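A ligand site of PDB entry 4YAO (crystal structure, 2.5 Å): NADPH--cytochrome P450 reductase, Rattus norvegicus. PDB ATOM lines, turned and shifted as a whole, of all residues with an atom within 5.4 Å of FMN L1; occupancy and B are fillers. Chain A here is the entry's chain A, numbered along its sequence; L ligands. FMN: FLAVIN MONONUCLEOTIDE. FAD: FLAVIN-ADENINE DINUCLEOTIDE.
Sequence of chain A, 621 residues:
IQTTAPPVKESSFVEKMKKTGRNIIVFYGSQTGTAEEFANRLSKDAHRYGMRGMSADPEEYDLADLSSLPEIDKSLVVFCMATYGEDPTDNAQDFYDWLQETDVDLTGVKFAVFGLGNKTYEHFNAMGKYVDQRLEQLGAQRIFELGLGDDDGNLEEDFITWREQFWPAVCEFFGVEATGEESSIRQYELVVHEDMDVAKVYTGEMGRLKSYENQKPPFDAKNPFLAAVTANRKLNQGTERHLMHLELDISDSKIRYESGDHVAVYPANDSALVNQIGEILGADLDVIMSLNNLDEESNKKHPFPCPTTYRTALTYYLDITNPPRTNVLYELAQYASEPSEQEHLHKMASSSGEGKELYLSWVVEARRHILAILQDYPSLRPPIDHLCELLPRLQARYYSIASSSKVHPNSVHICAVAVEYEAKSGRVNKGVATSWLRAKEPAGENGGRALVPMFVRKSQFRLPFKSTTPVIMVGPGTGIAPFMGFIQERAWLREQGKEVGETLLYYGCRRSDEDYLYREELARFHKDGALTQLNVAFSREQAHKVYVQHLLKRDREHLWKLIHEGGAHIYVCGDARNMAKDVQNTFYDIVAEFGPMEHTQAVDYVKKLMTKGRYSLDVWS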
ATOM      1  N   GLY A  29     -29.710 -20.406   4.961  1.00  0.00           N
ATOM      2  CA  GLY A  29     -28.331 -19.998   4.824  1.00  0.00           C
ATOM      3  C   GLY A  29     -28.405 -18.544   4.443  1.00  0.00           C
ATOM      4  O   GLY A  29     -28.889 -18.192   3.370  1.00  0.00           O
ATOM      5  N   SER A  30     -27.909 -17.690   5.327  1.00  0.00           N
ATOM      6  CA  SER A  30     -28.047 -16.257   5.129  1.00  0.00           C
ATOM      7  C   SER A  30     -26.772 -15.524   5.498  1.00  0.00           C
ATOM      8  O   SER A  30     -25.989 -15.980   6.333  1.00  0.00           O
ATOM      9  CB  SER A  30     -29.217 -15.711   5.962  1.00  0.00           C
ATOM     10  OG  SER A  30     -29.644 -14.453   5.475  1.00  0.00           O
ATOM     11  N   GLN A  31     -26.578 -14.382   4.861  1.00  0.00           N
ATOM     12  CA  GLN A  31     -25.414 -13.535   5.138  1.00  0.00           C
ATOM     13  C   GLN A  31     -25.886 -12.153   5.581  1.00  0.00           C
ATOM     14  O   GLN A  31     -25.265 -11.541   6.440  1.00  0.00           O
ATOM     15  CB  GLN A  31     -24.536 -13.400   3.899  1.00  0.00           C
ATOM     16  CG  GLN A  31     -23.115 -13.029   4.219  1.00  0.00           C
ATOM     17  CD  GLN A  31     -22.542 -13.960   5.243  1.00  0.00           C
ATOM     18  OE1 GLN A  31     -22.923 -13.917   6.406  1.00  0.00           O
ATOM     19  NE2 GLN A  31     -21.636 -14.832   4.801  1.00  0.00           N
ATOM     20  N   THR A  32     -26.959 -11.660   4.976  1.00  0.00           N
ATOM     21  CA  THR A  32     -27.498 -10.355   5.351  1.00  0.00           C
ATOM     22  C   THR A  32     -28.985 -10.465   5.700  1.00  0.00           C
ATOM     23  O   THR A  32     -29.783  -9.547   5.427  1.00  0.00           O
ATOM     24  CB  THR A  32     -27.291  -9.301   4.247  1.00  0.00           C
ATOM     25  OG1 THR A  32     -27.506  -9.895   2.953  1.00  0.00           O
ATOM     26  CG2 THR A  32     -25.864  -8.727   4.321  1.00  0.00           C
ATOM     27  N   GLY A  33     -29.350 -11.602   6.274  1.00  0.00           N
ATOM     28  CA  GLY A  33     -30.714 -11.848   6.716  1.00  0.00           C
ATOM     29  C   GLY A  33     -31.779 -12.310   5.744  1.00  0.00           C
ATOM     30  O   GLY A  33     -32.656 -13.074   6.147  1.00  0.00           O
ATOM     31  N   THR A  34     -31.680 -11.997   4.453  1.00  0.00           N
ATOM     32  CA  THR A  34     -32.799 -12.242   3.535  1.00  0.00           C
ATOM     33  C   THR A  34     -33.280 -13.701   3.387  1.00  0.00           C
ATOM     34  O   THR A  34     -34.477 -13.962   3.405  1.00  0.00           O
ATOM     35  CB  THR A  34     -32.482 -11.700   2.125  1.00  0.00           C
ATOM     36  OG1 THR A  34     -31.724 -10.498   2.236  1.00  0.00           O
ATOM     37  CG2 THR A  34     -33.767 -11.429   1.363  1.00  0.00           C
ATOM     38  N   ALA A  35     -32.349 -14.640   3.263  1.00  0.00           N
ATOM     39  CA  ALA A  35     -32.646 -16.073   3.296  1.00  0.00           C
ATOM     40  C   ALA A  35     -33.347 -16.458   4.579  1.00  0.00           C
ATOM     41  O   ALA A  35     -34.289 -17.258   4.565  1.00  0.00           O
ATOM     42  CB  ALA A  35     -31.367 -16.887   3.151  1.00  0.00           C
ATOM     43  N   GLU A  36     -32.879 -15.898   5.685  1.00  0.00           N
ATOM     44  CA  GLU A  36     -33.477 -16.204   6.964  1.00  0.00           C
ATOM     45  C   GLU A  36     -34.907 -15.672   6.963  1.00  0.00           C
ATOM     46  O   GLU A  36     -35.846 -16.429   7.172  1.00  0.00           O
ATOM     47  CB  GLU A  36     -32.666 -15.578   8.087  1.00  0.00           C
ATOM     48  CG  GLU A  36     -33.095 -16.061   9.457  1.00  0.00           C
ATOM     49  CD  GLU A  36     -32.498 -15.261  10.572  1.00  0.00           C
ATOM     50  OE1 GLU A  36     -32.623 -14.014  10.543  1.00  0.00           O
ATOM     51  OE2 GLU A  36     -31.924 -15.863  11.511  1.00  0.00           O
ATOM     52  N   ALA A  82     -28.422 -18.910   0.260  1.00  0.00           N
ATOM     53  CA  ALA A  82     -27.859 -17.802  -0.495  1.00  0.00           C
ATOM     54  C   ALA A  82     -26.434 -18.147  -0.907  1.00  0.00           C
ATOM     55  O   ALA A  82     -25.777 -18.951  -0.248  1.00  0.00           O
ATOM     56  CB  ALA A  82     -27.871 -16.547   0.356  1.00  0.00           C
ATOM     57  N   THR A  83     -25.964 -17.569  -2.000  1.00  0.00           N
ATOM     58  CA  THR A  83     -24.581 -17.802  -2.419  1.00  0.00           C
ATOM     59  C   THR A  83     -23.801 -16.517  -2.107  1.00  0.00           C
ATOM     60  O   THR A  83     -24.320 -15.423  -2.293  1.00  0.00           O
ATOM     61  CB  THR A  83     -24.439 -18.075  -3.948  1.00  0.00           C
ATOM     62  OG1 THR A  83     -25.264 -19.180  -4.311  1.00  0.00           O
ATOM     63  CG2 THR A  83     -23.020 -18.426  -4.296  1.00  0.00           C
ATOM     64  N   TYR A  84     -22.585 -16.671  -1.610  1.00  0.00           N
ATOM     65  CA  TYR A  84     -21.714 -15.526  -1.322  1.00  0.00           C
ATOM     66  C   TYR A  84     -20.341 -15.951  -1.836  1.00  0.00           C
ATOM     67  O   TYR A  84     -19.614 -16.693  -1.183  1.00  0.00           O
ATOM     68  CB  TYR A  84     -21.657 -15.223   0.178  1.00  0.00           C
ATOM     69  N   THR A  89     -22.381 -19.620   2.580  1.00  0.00           N
ATOM     70  CA  THR A  89     -22.294 -18.469   3.471  1.00  0.00           C
ATOM     71  C   THR A  89     -21.668 -19.054   4.738  1.00  0.00           C
ATOM     72  O   THR A  89     -21.691 -20.265   4.947  1.00  0.00           O
ATOM     73  CB  THR A  89     -23.683 -17.868   3.767  1.00  0.00           C
ATOM     74  OG1 THR A  89     -24.509 -18.853   4.404  1.00  0.00           O
ATOM     75  CG2 THR A  89     -24.353 -17.438   2.496  1.00  0.00           C
ATOM     76  N   LEU A 116     -31.208 -18.132  -3.215  1.00  0.00           N
ATOM     77  CA  LEU A 116     -31.152 -16.688  -3.406  1.00  0.00           C
ATOM     78  C   LEU A 116     -29.776 -16.368  -3.967  1.00  0.00           C
ATOM     79  O   LEU A 116     -28.745 -16.723  -3.390  1.00  0.00           O
ATOM     80  CB  LEU A 116     -31.319 -15.935  -2.081  1.00  0.00           C
ATOM     81  CG  LEU A 116     -32.549 -16.148  -1.224  1.00  0.00           C
ATOM     82  CD1 LEU A 116     -32.599 -17.575  -0.699  1.00  0.00           C
ATOM     83  CD2 LEU A 116     -32.503 -15.185  -0.050  1.00  0.00           C
ATOM     84  N   GLY A 117     -29.747 -15.692  -5.111  1.00  0.00           N
ATOM     85  CA  GLY A 117     -28.487 -15.337  -5.715  1.00  0.00           C
ATOM     86  C   GLY A 117     -28.656 -14.015  -6.430  1.00  0.00           C
ATOM     87  O   GLY A 117     -29.509 -13.210  -6.070  1.00  0.00           O
ATOM     88  N   ASN A 118     -27.839 -13.805  -7.450  1.00  0.00           N
ATOM     89  CA  ASN A 118     -27.860 -12.584  -8.253  1.00  0.00           C
ATOM     90  C   ASN A 118     -27.266 -13.020  -9.583  1.00  0.00           C
ATOM     91  O   ASN A 118     -26.181 -13.596  -9.613  1.00  0.00           O
ATOM     92  CB  ASN A 118     -27.007 -11.495  -7.592  1.00  0.00           C
ATOM     93  CG  ASN A 118     -27.031 -10.189  -8.354  1.00  0.00           C
ATOM     94  OD1 ASN A 118     -26.526 -10.095  -9.457  1.00  0.00           O
ATOM     95  ND2 ASN A 118     -27.625  -9.168  -7.744  1.00  0.00           N
ATOM     96  N   LYS A 119     -27.970 -12.758 -10.683  1.00  0.00           N
ATOM     97  CA  LYS A 119     -27.478 -13.196 -11.983  1.00  0.00           C
ATOM     98  C   LYS A 119     -26.173 -12.556 -12.463  1.00  0.00           C
ATOM     99  O   LYS A 119     -25.409 -13.183 -13.216  1.00  0.00           O
ATOM    100  CB  LYS A 119     -28.564 -13.019 -13.047  1.00  0.00           C
ATOM    101  CG  LYS A 119     -29.835 -13.822 -12.788  1.00  0.00           C
ATOM    102  CD  LYS A 119     -30.547 -14.142 -14.097  1.00  0.00           C
ATOM    103  CE  LYS A 119     -31.991 -14.588 -13.863  1.00  0.00           C
ATOM    104  NZ  LYS A 119     -32.915 -13.468 -13.480  1.00  0.00           N
ATOM    105  N   TYR A 121     -23.593 -12.380 -11.133  1.00  0.00           N
ATOM    106  CA  TYR A 121     -22.456 -13.153 -10.647  1.00  0.00           C
ATOM    107  C   TYR A 121     -22.043 -14.334 -11.514  1.00  0.00           C
ATOM    108  O   TYR A 121     -22.853 -14.933 -12.220  1.00  0.00           O
ATOM    109  CB  TYR A 121     -22.728 -13.602  -9.220  1.00  0.00           C
ATOM    110  CG  TYR A 121     -22.500 -12.494  -8.233  1.00  0.00           C
ATOM    111  CD1 TYR A 121     -21.211 -12.210  -7.769  1.00  0.00           C
ATOM    112  CD2 TYR A 121     -23.552 -11.692  -7.797  1.00  0.00           C
ATOM    113  CE1 TYR A 121     -20.974 -11.135  -6.898  1.00  0.00           C
ATOM    114  CE2 TYR A 121     -23.326 -10.621  -6.907  1.00  0.00           C
ATOM    115  CZ  TYR A 121     -22.036 -10.348  -6.471  1.00  0.00           C
ATOM    116  OH  TYR A 121     -21.793  -9.302  -5.602  1.00  0.00           O
ATOM    117  N   HIS A 123     -20.990 -17.456 -10.669  1.00  0.00           N
ATOM    118  CA  HIS A 123     -21.689 -18.662 -10.259  1.00  0.00           C
ATOM    119  C   HIS A 123     -23.064 -18.352  -9.634  1.00  0.00           C
ATOM    120  O   HIS A 123     -23.184 -18.195  -8.417  1.00  0.00           O
ATOM    121  CB  HIS A 123     -20.816 -19.445  -9.283  1.00  0.00           C
ATOM    122  CG  HIS A 123     -19.474 -19.812  -9.840  1.00  0.00           C
ATOM    123  ND1 HIS A 123     -19.314 -20.670 -10.903  1.00  0.00           N
ATOM    124  CD2 HIS A 123     -18.220 -19.413  -9.491  1.00  0.00           C
ATOM    125  CE1 HIS A 123     -18.024 -20.797 -11.191  1.00  0.00           C
ATOM    126  NE2 HIS A 123     -17.346 -20.042 -10.345  1.00  0.00           N
ATOM    127  N   PHE A 124     -24.092 -18.302 -10.474  1.00  0.00           N
ATOM    128  CA  PHE A 124     -25.450 -17.989 -10.036  1.00  0.00           C
ATOM    129  C   PHE A 124     -26.119 -19.066  -9.189  1.00  0.00           C
ATOM    130  O   PHE A 124     -26.278 -20.214  -9.605  1.00  0.00           O
ATOM    131  CB  PHE A 124     -26.304 -17.690 -11.259  1.00  0.00           C
ATOM    132  CG  PHE A 124     -27.711 -17.330 -10.939  1.00  0.00           C
ATOM    133  CD1 PHE A 124     -27.990 -16.426  -9.911  1.00  0.00           C
ATOM    134  CD2 PHE A 124     -28.775 -17.877 -11.672  1.00  0.00           C
ATOM    135  CE1 PHE A 124     -29.292 -16.060  -9.609  1.00  0.00           C
ATOM    136  CE2 PHE A 124     -30.087 -17.526 -11.379  1.00  0.00           C
ATOM    137  CZ  PHE A 124     -30.348 -16.612 -10.344  1.00  0.00           C
ATOM    138  N   ASN A 125     -26.538 -18.676  -7.984  1.00  0.00           N
ATOM    139  CA  ASN A 125     -27.204 -19.588  -7.055  1.00  0.00           C
ATOM    140  C   ASN A 125     -26.466 -20.906  -6.874  1.00  0.00           C
ATOM    141  O   ASN A 125     -27.068 -21.922  -6.539  1.00  0.00           O
ATOM    142  CB  ASN A 125     -28.648 -19.881  -7.509  1.00  0.00           C
ATOM    143  CG  ASN A 125     -29.664 -18.926  -6.893  1.00  0.00           C
ATOM    144  OD1 ASN A 125     -29.773 -18.832  -5.672  1.00  0.00           O
ATOM    145  ND2 ASN A 125     -30.410 -18.223  -7.736  1.00  0.00           N
ATOM    146  N   ALA A 126     -25.148 -20.887  -7.075  1.00  0.00           N
ATOM    147  CA  ALA A 126     -24.344 -22.095  -6.955  1.00  0.00           C
ATOM    148  C   ALA A 126     -24.672 -22.932  -5.714  1.00  0.00           C
ATOM    149  O   ALA A 126     -24.706 -24.167  -5.776  1.00  0.00           O
ATOM    150  CB  ALA A 126     -22.875 -21.731  -6.957  1.00  0.00           C
ATOM    151  N   ASP A 151     -31.637 -11.534  -7.320  1.00  0.00           N
ATOM    152  CA  ASP A 151     -31.649 -10.212  -6.705  1.00  0.00           C
ATOM    153  C   ASP A 151     -31.282  -9.083  -7.663  1.00  0.00           C
ATOM    154  O   ASP A 151     -31.128  -7.942  -7.252  1.00  0.00           O
ATOM    155  CB  ASP A 151     -30.720 -10.195  -5.496  1.00  0.00           C
ATOM    156  CG  ASP A 151     -31.109  -9.129  -4.504  1.00  0.00           C
ATOM    157  OD1 ASP A 151     -32.311  -8.783  -4.446  1.00  0.00           O
ATOM    158  OD2 ASP A 151     -30.208  -8.639  -3.784  1.00  0.00           O
ATOM    159  N   LEU A 155     -35.994 -10.261  -6.077  1.00  0.00           N
ATOM    160  CA  LEU A 155     -36.022 -11.511  -5.328  1.00  0.00           C
ATOM    161  C   LEU A 155     -37.347 -11.739  -4.637  1.00  0.00           C
ATOM    162  O   LEU A 155     -37.845 -12.860  -4.587  1.00  0.00           O
ATOM    163  CB  LEU A 155     -34.881 -11.540  -4.307  1.00  0.00           C
ATOM    164  CG  LEU A 155     -34.598 -12.904  -3.677  1.00  0.00           C
ATOM    165  CD1 LEU A 155     -34.323 -13.921  -4.760  1.00  0.00           C
ATOM    166  CD2 LEU A 155     -33.409 -12.797  -2.764  1.00  0.00           C
ATOM    167  N   VAL A 619     -16.397  -6.745  -6.651  1.00  0.00           N
ATOM    168  CA  VAL A 619     -17.421  -5.867  -7.173  1.00  0.00           C
ATOM    169  C   VAL A 619     -18.652  -5.944  -6.295  1.00  0.00           C
ATOM    170  O   VAL A 619     -18.923  -6.975  -5.669  1.00  0.00           O
ATOM    171  CB  VAL A 619     -17.788  -6.242  -8.601  1.00  0.00           C
ATOM    172  CG1 VAL A 619     -16.531  -6.246  -9.460  1.00  0.00           C
ATOM    173  CG2 VAL A 619     -18.466  -7.612  -8.628  1.00  0.00           C
HETATM  174  N1  FMN L   1     -25.246 -14.356  -5.681  1.00  0.00           N
HETATM  175  C2  FMN L   1     -25.033 -15.425  -6.461  1.00  0.00           C
HETATM  176  O2  FMN L   1     -25.963 -15.979  -7.059  1.00  0.00           O
HETATM  177  N3  FMN L   1     -23.741 -15.884  -6.564  1.00  0.00           N
HETATM  178  C4  FMN L   1     -22.607 -15.344  -5.948  1.00  0.00           C
HETATM  179  O4  FMN L   1     -21.565 -15.931  -6.211  1.00  0.00           O
HETATM  180  C4A FMN L   1     -22.813 -14.196  -5.128  1.00  0.00           C
HETATM  181  N5  FMN L   1     -21.693 -13.621  -4.508  1.00  0.00           N
HETATM  182  C5A FMN L   1     -21.982 -12.504  -3.725  1.00  0.00           C
HETATM  183  C6  FMN L   1     -20.846 -11.902  -3.101  1.00  0.00           C
HETATM  184  C7  FMN L   1     -20.984 -10.752  -2.294  1.00  0.00           C
HETATM  185  C7M FMN L   1     -19.669 -10.203  -1.674  1.00  0.00           C
HETATM  186  C8  FMN L   1     -22.326 -10.133  -2.063  1.00  0.00           C
HETATM  187  C8M FMN L   1     -22.587  -9.021  -1.301  1.00  0.00           C
HETATM  188  C9  FMN L   1     -23.435 -10.713  -2.662  1.00  0.00           C
HETATM  189  C9A FMN L   1     -23.316 -11.905  -3.513  1.00  0.00           C
HETATM  190  N10 FMN L   1     -24.441 -12.570  -4.201  1.00  0.00           N
HETATM  191  C10 FMN L   1     -24.179 -13.761  -5.035  1.00  0.00           C
HETATM  192  C1' FMN L   1     -25.817 -12.082  -4.071  1.00  0.00           C
HETATM  193  C2' FMN L   1     -26.615 -12.708  -2.884  1.00  0.00           C
HETATM  194  O2' FMN L   1     -26.635 -14.169  -3.055  1.00  0.00           O
HETATM  195  C3' FMN L   1     -28.052 -12.161  -2.833  1.00  0.00           C
HETATM  196  O3' FMN L   1     -27.954 -10.728  -2.655  1.00  0.00           O
HETATM  197  C4' FMN L   1     -28.795 -12.859  -1.630  1.00  0.00           C
HETATM  198  O4' FMN L   1     -30.135 -12.277  -1.753  1.00  0.00           O
HETATM  199  C5' FMN L   1     -28.295 -12.462  -0.254  1.00  0.00           C
HETATM  200  O5' FMN L   1     -29.003 -13.219   0.802  1.00  0.00           O
HETATM  201  P   FMN L   1     -28.791 -13.108   2.361  1.00  0.00           P
HETATM  202  O1P FMN L   1     -29.275 -11.806   2.865  1.00  0.00           O
HETATM  203  O2P FMN L   1     -27.302 -13.527   2.538  1.00  0.00           O
HETATM  204  O3P FMN L   1     -29.803 -14.220   2.880  1.00  0.00           O
HETATM  205  PA  FAD L   2     -28.326   2.038   2.254  1.00  0.00           P
HETATM  206  O1A FAD L   2     -29.292   2.568   3.250  1.00  0.00           O
HETATM  207  O2A FAD L   2     -27.830   0.657   2.386  1.00  0.00           O
HETATM  208  O5B FAD L   2     -29.009   2.194   0.802  1.00  0.00           O
HETATM  209  C5B FAD L   2     -28.432   1.555  -0.339  1.00  0.00           C
HETATM  210  C4B FAD L   2     -29.508   1.469  -1.420  1.00  0.00           C
HETATM  211  O4B FAD L   2     -30.007   2.765  -1.773  1.00  0.00           O
HETATM  212  C3B FAD L   2     -28.923   0.971  -2.725  1.00  0.00           C
HETATM  213  O3B FAD L   2     -28.700  -0.449  -2.624  1.00  0.00           O
HETATM  214  C2B FAD L   2     -30.137   1.252  -3.586  1.00  0.00           C
HETATM  215  O2B FAD L   2     -31.180   0.308  -3.280  1.00  0.00           O
HETATM  216  C1B FAD L   2     -30.531   2.636  -3.099  1.00  0.00           C
HETATM  217  N9A FAD L   2     -29.905   3.707  -3.909  1.00  0.00           N
HETATM  218  C8A FAD L   2     -28.517   4.196  -3.781  1.00  0.00           C
HETATM  219  N7A FAD L   2     -28.586   5.392  -4.647  1.00  0.00           N
HETATM  220  C5A FAD L   2     -29.771   5.391  -5.262  1.00  0.00           C
HETATM  221  C6A FAD L   2     -30.275   6.275  -6.121  1.00  0.00           C
HETATM  222  N6A FAD L   2     -29.534   7.346  -6.368  1.00  0.00           N
HETATM  223  N1A FAD L   2     -31.426   6.063  -6.779  1.00  0.00           N
HETATM  224  C2A FAD L   2     -32.112   4.851  -6.561  1.00  0.00           C
HETATM  225  N3A FAD L   2     -31.559   3.956  -5.646  1.00  0.00           N
HETATM  226  C4A FAD L   2     -30.412   4.247  -5.005  1.00  0.00           C
HETATM  227  N1  FAD L   2     -18.988   1.149  -0.831  1.00  0.00           N
HETATM  228  C2  FAD L   2     -17.914   2.054  -0.805  1.00  0.00           C
HETATM  229  O2  FAD L   2     -18.113   3.247  -1.027  1.00  0.00           O
HETATM  230  N3  FAD L   2     -16.609   1.585  -0.653  1.00  0.00           N
HETATM  231  C4  FAD L   2     -16.368   0.212  -0.537  1.00  0.00           C
HETATM  232  O4  FAD L   2     -15.269  -0.160  -0.127  1.00  0.00           O
HETATM  233  C4X FAD L   2     -17.427  -0.682  -0.578  1.00  0.00           C
HETATM  234  N5  FAD L   2     -17.199  -2.005  -0.652  1.00  0.00           N
HETATM  235  C5X FAD L   2     -18.220  -2.863  -0.659  1.00  0.00           C
HETATM  236  C6  FAD L   2     -17.977  -4.230  -0.629  1.00  0.00           C
HETATM  237  C7  FAD L   2     -19.023  -5.133  -0.482  1.00  0.00           C
HETATM  238  C7M FAD L   2     -18.743  -6.465  -0.207  1.00  0.00           C
HETATM  239  C8  FAD L   2     -20.325  -4.663  -0.409  1.00  0.00           C
HETATM  240  C8M FAD L   2     -21.391  -5.561  -0.340  1.00  0.00           C
HETATM  241  C9  FAD L   2     -20.579  -3.290  -0.460  1.00  0.00           C
HETATM  242  C9A FAD L   2     -19.533  -2.397  -0.566  1.00  0.00           C
HETATM  243  N10 FAD L   2     -19.757  -1.072  -0.547  1.00  0.00           N
HETATM  244  C10 FAD L   2     -18.733  -0.218  -0.721  1.00  0.00           C
HETATM  245  C1' FAD L   2     -21.135  -0.537  -0.451  1.00  0.00           C
HETATM  246  C2' FAD L   2     -21.531  -0.321   1.008  1.00  0.00           C
HETATM  247  O2' FAD L   2     -21.460  -1.552   1.724  1.00  0.00           O
HETATM  248  C3' FAD L   2     -22.945   0.250   1.107  1.00  0.00           C
HETATM  249  O3' FAD L   2     -23.803  -0.484   0.227  1.00  0.00           O
HETATM  250  C4' FAD L   2     -22.948   1.730   0.714  1.00  0.00           C
HETATM  251  O4' FAD L   2     -21.968   2.419   1.507  1.00  0.00           O
HETATM  252  C5' FAD L   2     -24.332   2.338   0.946  1.00  0.00           C
HETATM  253  O5' FAD L   2     -24.779   1.983   2.252  1.00  0.00           O
HETATM  254  P   FAD L   2     -25.784   2.909   3.113  1.00  0.00           P
HETATM  255  O1P FAD L   2     -25.193   4.258   3.254  1.00  0.00           O
HETATM  256  O2P FAD L   2     -26.124   2.155   4.338  1.00  0.00           O
HETATM  257  O3P FAD L   2     -27.075   3.041   2.159  1.00  0.00           O
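O3P of FMN L1 lies within hydrogen-bond range of OG of Ser 30 (2.6 Å). The backbone carbonyl oxygen (O) of Thr 83 sits at hydrogen-bond distance from an oxygen (O2') of FMN L1. O1P of FMN L1 lies within hydrogen-bond range of N of Thr 34 (2.9 Å). O2P of FMN L1 lies within hydrogen-bond range of N of Gln 31, 2.6 Å away. N of Gly 33 is in hydrogen-bond range of O1P of FMN L1, 3.4 Å away. OG1 of Thr 34 is in hydrogen-bond range of O1P of FMN L1. A nitrogen (N3) of FMN L1 lies within hydrogen-bond range of the backbone carbonyl oxygen of His 123 (3.0 Å). The side-chain hydroxyl (OG1) of Thr 32 lies within hydrogen-bond range of an oxygen (O1P) of FMN L1 (2.6 Å). The backbone NH (N) of Asn 118 lies within hydrogen-bond range of an oxygen (O2) of FMN L1 (2.9 Å). N of Ala 35 sits at hydrogen-bond distance from O3P of FMN L1, at 2.6 Å. An oxygen (O2P) of FMN L1 lies within hydrogen-bond range of the backbone NH (N) of Thr 32, at 3.1 Å. N of Asn 125 is in hydrogen-bond range of O2 of FMN L1. The backbone carbonyl oxygen (O) of Leu 116 lies within hydrogen-bond range of an oxygen (O2') of FMN L1, at 3.3 Å. OD2 of Asp 151 sits at hydrogen-bond distance from O3' of FMN L1 (3.3 Å).
O of Gly 117 is in hydrogen-bond range of N of Asp 151, 3.0 Å away. OG1 of Thr 83 is in hydrogen-bond range of N of Ala 126 (3.3 Å). The backbone carbonyl oxygen of Leu 116 lies within hydrogen-bond range of the backbone NH of Thr 83 (3.2 Å). The backbone NH (N) of Leu 116 lies within hydrogen-bond range of the side-chain amide oxygen (OD1) of Asn 125, 2.9 Å away. The backbone NH (N) of Ala 35 sits at hydrogen-bond distance from the side-chain hydroxyl (OG) of Ser 30, 3.5 Å away. The side-chain amide oxygen (OD1) of Asn 125 sits at hydrogen-bond distance from the backbone NH (N) of Gly 117 (3.2 Å). N of Ala 82 lies within hydrogen-bond range of O of Gly 29. N of Gly 33 lies within hydrogen-bond range of OG of Ser 30 (3.0 Å).
Ala 82 touches FMN L1 (CB to O5', 3.5 Å). Tyr 84 touches FMN L1 (CA to N5, 3.7 Å). Gly 117 touches FMN L1. Tyr 121 touches FMN L1 (CZ to C5A, 3.5 Å). Phe 124 touches FMN L1. Leu 155 touches FMN L1 (CD2 to O4', 3.5 Å). Of the 24 residues printed, 18 come within 4 Å of FMN L1. The nearest printed residue that does not touch FMN L1 is Gly 29 (4.1 Å).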
